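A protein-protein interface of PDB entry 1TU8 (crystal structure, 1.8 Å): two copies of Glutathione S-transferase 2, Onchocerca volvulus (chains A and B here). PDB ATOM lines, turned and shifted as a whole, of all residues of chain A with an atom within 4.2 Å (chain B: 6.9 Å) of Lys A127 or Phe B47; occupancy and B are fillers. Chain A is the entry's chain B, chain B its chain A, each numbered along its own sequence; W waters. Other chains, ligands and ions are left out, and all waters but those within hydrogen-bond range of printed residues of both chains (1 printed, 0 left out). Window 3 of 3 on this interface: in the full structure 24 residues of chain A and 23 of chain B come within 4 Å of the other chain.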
ATOM      1  N   MET A  89       7.926   2.311  17.534  1.00  0.00           N
ATOM      2  CA  MET A  89       8.812   3.056  18.410  1.00  0.00           C
ATOM      3  C   MET A  89       9.047   4.493  17.924  1.00  0.00           C
ATOM      4  O   MET A  89       8.948   5.441  18.698  1.00  0.00           O
ATOM      5  CB  MET A  89      10.135   2.304  18.525  1.00  0.00           C
ATOM      6  CG  MET A  89      11.107   2.879  19.505  1.00  0.00           C
ATOM      7  SD  MET A  89      12.643   1.902  19.460  1.00  0.00           S
ATOM      8  CE  MET A  89      13.589   2.904  18.296  1.00  0.00           C
ATOM      9  N   GLY A  93       7.675   8.103  19.649  1.00  0.00           N
ATOM     10  CA  GLY A  93       8.518   9.244  19.941  1.00  0.00           C
ATOM     11  C   GLY A  93       7.920  10.522  19.380  1.00  0.00           C
ATOM     12  O   GLY A  93       7.942  11.563  20.027  1.00  0.00           O
ATOM     13  N   GLY A 123      16.924  19.685  21.452  1.00  0.00           N
ATOM     14  CA  GLY A 123      17.306  18.387  21.985  1.00  0.00           C
ATOM     15  C   GLY A 123      16.361  17.265  21.569  1.00  0.00           C
ATOM     16  O   GLY A 123      16.795  16.143  21.308  1.00  0.00           O
ATOM     17  N   GLU A 124      15.072  17.570  21.476  1.00  0.00           N
ATOM     18  CA  GLU A 124      14.103  16.574  21.020  1.00  0.00           C
ATOM     19  C   GLU A 124      14.272  16.256  19.540  1.00  0.00           C
ATOM     20  O   GLU A 124      14.256  15.087  19.152  1.00  0.00           O
ATOM     21  CB  GLU A 124      12.679  17.032  21.307  1.00  0.00           C
ATOM     22  CG  GLU A 124      12.372  17.213  22.782  1.00  0.00           C
ATOM     23  CD  GLU A 124      12.658  15.971  23.611  1.00  0.00           C
ATOM     24  OE1 GLU A 124      13.198  16.124  24.723  1.00  0.00           O
ATOM     25  OE2 GLU A 124      12.350  14.851  23.154  1.00  0.00           O
ATOM     26  N   LEU A 125      14.418  17.283  18.711  1.00  0.00           N
ATOM     27  CA  LEU A 125      14.632  17.072  17.274  1.00  0.00           C
ATOM     28  C   LEU A 125      15.915  16.282  17.011  1.00  0.00           C
ATOM     29  O   LEU A 125      15.951  15.440  16.120  1.00  0.00           O
ATOM     30  CB  LEU A 125      14.641  18.400  16.521  1.00  0.00           C
ATOM     31  CG  LEU A 125      13.297  19.134  16.481  1.00  0.00           C
ATOM     32  CD1 LEU A 125      13.471  20.532  15.911  1.00  0.00           C
ATOM     33  CD2 LEU A 125      12.257  18.361  15.665  1.00  0.00           C
ATOM     34  N   ALA A 126      16.950  16.518  17.814  1.00  0.00           N
ATOM     35  CA  ALA A 126      18.232  15.823  17.651  1.00  0.00           C
ATOM     36  C   ALA A 126      18.098  14.298  17.781  1.00  0.00           C
ATOM     37  O   ALA A 126      18.784  13.558  17.083  1.00  0.00           O
ATOM     38  CB  ALA A 126      19.252  16.349  18.646  1.00  0.00           C
ATOM     39  N   LYS A 127      17.199  13.849  18.655  1.00  0.00           N
ATOM     40  CA  LYS A 127      16.886  12.420  18.794  1.00  0.00           C
ATOM     41  C   LYS A 127      16.348  11.816  17.493  1.00  0.00           C
ATOM     42  O   LYS A 127      16.737  10.716  17.107  1.00  0.00           O
ATOM     43  CB  LYS A 127      15.859  12.204  19.905  1.00  0.00           C
ATOM     44  CG  LYS A 127      16.365  12.508  21.303  1.00  0.00           C
ATOM     45  CD  LYS A 127      15.214  12.777  22.237  1.00  0.00           C
ATOM     46  CE  LYS A 127      15.668  13.100  23.656  1.00  0.00           C
ATOM     47  NZ  LYS A 127      14.465  13.189  24.550  1.00  0.00           N
ATOM     48  N   PHE A 128      15.462  12.545  16.820  1.00  0.00           N
ATOM     49  CA  PHE A 128      14.927  12.109  15.533  1.00  0.00           C
ATOM     50  C   PHE A 128      15.952  12.147  14.396  1.00  0.00           C
ATOM     51  O   PHE A 128      15.972  11.260  13.556  1.00  0.00           O
ATOM     52  CB  PHE A 128      13.711  12.957  15.161  1.00  0.00           C
ATOM     53  CG  PHE A 128      12.572  12.812  16.134  1.00  0.00           C
ATOM     54  CD1 PHE A 128      12.279  13.819  17.032  1.00  0.00           C
ATOM     55  CD2 PHE A 128      11.827  11.645  16.174  1.00  0.00           C
ATOM     56  CE1 PHE A 128      11.235  13.683  17.940  1.00  0.00           C
ATOM     57  CE2 PHE A 128      10.779  11.502  17.078  1.00  0.00           C
ATOM     58  CZ  PHE A 128      10.488  12.523  17.959  1.00  0.00           C
ATOM     59  N   GLU A 129      16.779  13.184  14.370  1.00  0.00           N
ATOM     60  CA  GLU A 129      17.829  13.327  13.358  1.00  0.00           C
ATOM     61  C   GLU A 129      18.745  12.095  13.386  1.00  0.00           C
ATOM     62  O   GLU A 129      19.074  11.524  12.334  1.00  0.00           O
ATOM     63  CB  GLU A 129      18.616  14.630  13.598  1.00  0.00           C
ATOM     64  CG  GLU A 129      19.768  14.907  12.625  1.00  0.00           C
ATOM     65  CD  GLU A 129      19.327  15.441  11.269  1.00  0.00           C
ATOM     66  OE1 GLU A 129      18.111  15.632  11.036  1.00  0.00           O
ATOM     67  OE2 GLU A 129      20.204  15.662  10.407  1.00  0.00           O
ATOM     68  N   LYS A 130      19.126  11.676  14.589  1.00  0.00           N
ATOM     69  CA  LYS A 130      19.951  10.487  14.779  1.00  0.00           C
ATOM     70  C   LYS A 130      19.218   9.191  14.394  1.00  0.00           C
ATOM     71  O   LYS A 130      19.785   8.312  13.734  1.00  0.00           O
ATOM     72  CB  LYS A 130      20.444  10.403  16.232  1.00  0.00           C
ATOM     73  CG  LYS A 130      21.422   9.245  16.460  1.00  0.00           C
ATOM     74  CD  LYS A 130      22.054   9.247  17.835  1.00  0.00           C
ATOM     75  CE  LYS A 130      22.931   8.002  17.988  1.00  0.00           C
ATOM     76  NZ  LYS A 130      23.497   7.853  19.364  1.00  0.00           N
ATOM     77  N   LEU A 131      17.953   9.082  14.805  1.00  0.00           N
ATOM     78  CA  LEU A 131      17.160   7.889  14.539  1.00  0.00           C
ATOM     79  C   LEU A 131      16.879   7.733  13.044  1.00  0.00           C
ATOM     80  O   LEU A 131      17.044   6.645  12.483  1.00  0.00           O
ATOM     81  CB  LEU A 131      15.847   7.938  15.339  1.00  0.00           C
ATOM     82  CG  LEU A 131      15.204   6.595  15.693  1.00  0.00           C
ATOM     83  CD1 LEU A 131      16.211   5.652  16.360  1.00  0.00           C
ATOM     84  CD2 LEU A 131      13.995   6.831  16.590  1.00  0.00           C
ATOM     85  N   LYS B  42      21.869   7.893  30.095  1.00  0.00           N
ATOM     86  CA  LYS B  42      20.726   8.469  29.381  1.00  0.00           C
ATOM     87  C   LYS B  42      20.867   8.451  27.856  1.00  0.00           C
ATOM     88  O   LYS B  42      19.916   8.119  27.150  1.00  0.00           O
ATOM     89  CB  LYS B  42      20.461   9.902  29.877  1.00  0.00           C
ATOM     90  CG  LYS B  42      19.430  10.693  29.071  1.00  0.00           C
ATOM     91  CD  LYS B  42      18.913  11.913  29.837  1.00  0.00           C
ATOM     92  CE  LYS B  42      17.892  12.715  29.023  1.00  0.00           C
ATOM     93  NZ  LYS B  42      16.474  12.267  29.236  1.00  0.00           N
ATOM     94  N   GLN B  44      22.283   6.431  25.926  1.00  0.00           N
ATOM     95  CA  GLN B  44      22.235   5.097  25.327  1.00  0.00           C
ATOM     96  C   GLN B  44      20.844   4.732  24.784  1.00  0.00           C
ATOM     97  O   GLN B  44      20.704   3.759  24.048  1.00  0.00           O
ATOM     98  CB  GLN B  44      22.657   4.044  26.345  1.00  0.00           C
ATOM     99  CG  GLN B  44      24.098   4.171  26.833  1.00  0.00           C
ATOM    100  CD  GLN B  44      24.444   3.110  27.861  1.00  0.00           C
ATOM    101  OE1 GLN B  44      23.804   2.061  27.913  1.00  0.00           O
ATOM    102  NE2 GLN B  44      25.445   3.384  28.688  1.00  0.00           N
ATOM    103  N   PHE B  45      19.825   5.505  25.164  1.00  0.00           N
ATOM    104  CA  PHE B  45      18.442   5.235  24.773  1.00  0.00           C
ATOM    105  C   PHE B  45      17.984   6.219  23.705  1.00  0.00           C
ATOM    106  O   PHE B  45      18.327   7.392  23.748  1.00  0.00           O
ATOM    107  CB  PHE B  45      17.554   5.269  26.017  1.00  0.00           C
ATOM    108  CG  PHE B  45      18.028   4.326  27.081  1.00  0.00           C
ATOM    109  CD1 PHE B  45      18.832   4.774  28.124  1.00  0.00           C
ATOM    110  CD2 PHE B  45      17.761   2.969  26.976  1.00  0.00           C
ATOM    111  CE1 PHE B  45      19.312   3.883  29.081  1.00  0.00           C
ATOM    112  CE2 PHE B  45      18.239   2.076  27.930  1.00  0.00           C
ATOM    113  CZ  PHE B  45      19.015   2.536  28.980  1.00  0.00           C
ATOM    114  N   GLN B  46      17.202   5.719  22.758  1.00  0.00           N
ATOM    115  CA  GLN B  46      16.886   6.444  21.526  1.00  0.00           C
ATOM    116  C   GLN B  46      16.152   7.775  21.768  1.00  0.00           C
ATOM    117  O   GLN B  46      16.308   8.720  20.990  1.00  0.00           O
ATOM    118  CB  GLN B  46      16.090   5.548  20.564  1.00  0.00           C
ATOM    119  CG  GLN B  46      16.896   4.381  19.944  1.00  0.00           C
ATOM    120  CD  GLN B  46      16.689   3.039  20.650  1.00  0.00           C
ATOM    121  OE1 GLN B  46      16.620   1.987  20.002  1.00  0.00           O
ATOM    122  NE2 GLN B  46      16.601   3.072  21.961  1.00  0.00           N
ATOM    123  N   PHE B  47      15.370   7.859  22.841  1.00  0.00           N
ATOM    124  CA  PHE B  47      14.678   9.104  23.208  1.00  0.00           C
ATOM    125  C   PHE B  47      15.117   9.628  24.580  1.00  0.00           C
ATOM    126  O   PHE B  47      14.476  10.514  25.158  1.00  0.00           O
ATOM    127  CB  PHE B  47      13.147   8.928  23.145  1.00  0.00           C
ATOM    128  CG  PHE B  47      12.647   8.569  21.782  1.00  0.00           C
ATOM    129  CD1 PHE B  47      12.095   7.312  21.530  1.00  0.00           C
ATOM    130  CD2 PHE B  47      12.749   9.475  20.732  1.00  0.00           C
ATOM    131  CE1 PHE B  47      11.653   6.975  20.270  1.00  0.00           C
ATOM    132  CE2 PHE B  47      12.310   9.136  19.453  1.00  0.00           C
ATOM    133  CZ  PHE B  47      11.761   7.882  19.224  1.00  0.00           C
ATOM    134  N   GLY B  48      16.221   9.085  25.093  1.00  0.00           N
ATOM    135  CA  GLY B  48      16.758   9.483  26.381  1.00  0.00           C
ATOM    136  C   GLY B  48      15.889   9.105  27.569  1.00  0.00           C
ATOM    137  O   GLY B  48      15.961   9.738  28.621  1.00  0.00           O
ATOM    138  N   GLN B  49      15.069   8.070  27.403  1.00  0.00           N
ATOM    139  CA  GLN B  49      14.070   7.705  28.407  1.00  0.00           C
ATOM    140  C   GLN B  49      13.866   6.199  28.510  1.00  0.00           C
ATOM    141  O   GLN B  49      14.262   5.441  27.625  1.00  0.00           O
ATOM    142  CB  GLN B  49      12.734   8.391  28.091  1.00  0.00           C
ATOM    143  CG  GLN B  49      12.760   9.891  28.351  1.00  0.00           C
ATOM    144  CD  GLN B  49      11.385  10.501  28.565  1.00  0.00           C
ATOM    145  OE1 GLN B  49      11.176  11.258  29.521  1.00  0.00           O
ATOM    146  NE2 GLN B  49      10.449  10.186  27.684  1.00  0.00           N
ATOM    147  N   LEU B  50      13.242   5.801  29.613  1.00  0.00           N
ATOM    148  CA  LEU B  50      12.912   4.414  29.929  1.00  0.00           C
ATOM    149  C   LEU B  50      11.387   4.281  30.020  1.00  0.00           C
ATOM    150  O   LEU B  50      10.705   5.297  30.220  1.00  0.00           O
ATOM    151  CB  LEU B  50      13.548   4.050  31.268  1.00  0.00           C
ATOM    152  CG  LEU B  50      15.067   4.195  31.354  1.00  0.00           C
ATOM    153  CD1 LEU B  50      15.535   3.852  32.761  1.00  0.00           C
ATOM    154  CD2 LEU B  50      15.753   3.301  30.328  1.00  0.00           C
ATOM    155  N   VAL B  61      12.810   0.891  22.940  1.00  0.00           N
ATOM    156  CA  VAL B  61      12.212   1.830  23.879  1.00  0.00           C
ATOM    157  C   VAL B  61      10.764   2.094  23.475  1.00  0.00           C
ATOM    158  O   VAL B  61      10.297   1.578  22.456  1.00  0.00           O
ATOM    159  CB  VAL B  61      13.009   3.157  23.988  1.00  0.00           C
ATOM    160  CG1 VAL B  61      14.397   2.908  24.605  1.00  0.00           C
ATOM    161  CG2 VAL B  61      13.130   3.852  22.645  1.00  0.00           C
ATOM    162  N   GLN B  62      10.071   2.863  24.315  1.00  0.00           N
ATOM    163  CA  GLN B  62       8.663   3.240  24.166  1.00  0.00           C
ATOM    164  C   GLN B  62       7.755   2.111  24.659  1.00  0.00           C
ATOM    165  O   GLN B  62       7.605   1.084  23.993  1.00  0.00           O
ATOM    166  CB  GLN B  62       8.316   3.674  22.725  1.00  0.00           C
ATOM    167  CG  GLN B  62       8.921   5.006  22.301  1.00  0.00           C
ATOM    168  CD  GLN B  62       8.291   6.223  22.975  1.00  0.00           C
ATOM    169  OE1 GLN B  62       8.804   7.344  22.852  1.00  0.00           O
ATOM    170  NE2 GLN B  62       7.208   6.011  23.692  1.00  0.00           N
HETATM  171  O   HOH W   1      17.925   9.066  18.829  1.00  0.00           O
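The side-chain amino group (NZ) of Lys A127 is in hydrogen-bond range of the backbone carbonyl oxygen (O) of Phe B47. The side-chain sulfur (SD) of Met A89 sits at hydrogen-bond distance from the backbone NH (N) of Val B61. The backbone NH (N) of Gly A93 lies within hydrogen-bond range of the side-chain amide oxygen (OE1) of Gln B62 (3.5 Å).
The side-chain carboxylate (OE2) of Glu A124 is in salt-bridge range of the side-chain amino group (NZ) of Lys A127 (3.0 Å).
Among the printed residues, merely in contact across the chains: Met A89 with Phe B47, Gly A93 with Phe B47, Met A89 with Gln B46, Leu A131 with Phe B47, Met A89 with Gln B62, Lys A127 with Gln B46, Phe A128 with Phe B47 and Leu A131 with Gln B46.
Of chain B, only Gln B46 and Phe B47 come within 4 Å of Lys A127. Of chain A, only Met A89 (3.5 Å), Gly A93 (3.6 Å), Lys A127 (2.7 Å), Phe A128 (3.7 Å) and Leu A131 (3.6 Å) come within 4 Å of Phe B47. Printed residues of chain B within 4 Å of Gly A93: Phe B47 (3.6 Å) and Gln B62 (3.5 Å). Printed residues of chain B within 4 Å of Met A89: Gln B46 (3.6 Å), Phe B47 (3.5 Å), Val B61 (3.3 Å) and Gln B62 (3.6 Å). Printed residues of chain A within 4 Å of Val B61: Met A89 (3.3 Å). Glu A124 touches none of the printed residues of chain B.
Printed residues of chain A that touch a printed residue of chain B: Met A89, Gly A93, Lys A127, Phe A128 and Leu A131. Along chain A the printed residues that touch a printed residue of chain B span positions 89 to 131. Of the 10 printed residues of chain B, 4 touch a printed residue of chain A. Among the printed residues, 11 pairs touch across the chains.
No position is printed for both chains.
Water W1 lies within hydrogen-bond range of O of Lys A127 (2.7 Å) and O of Gln B46 (2.7 Å).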
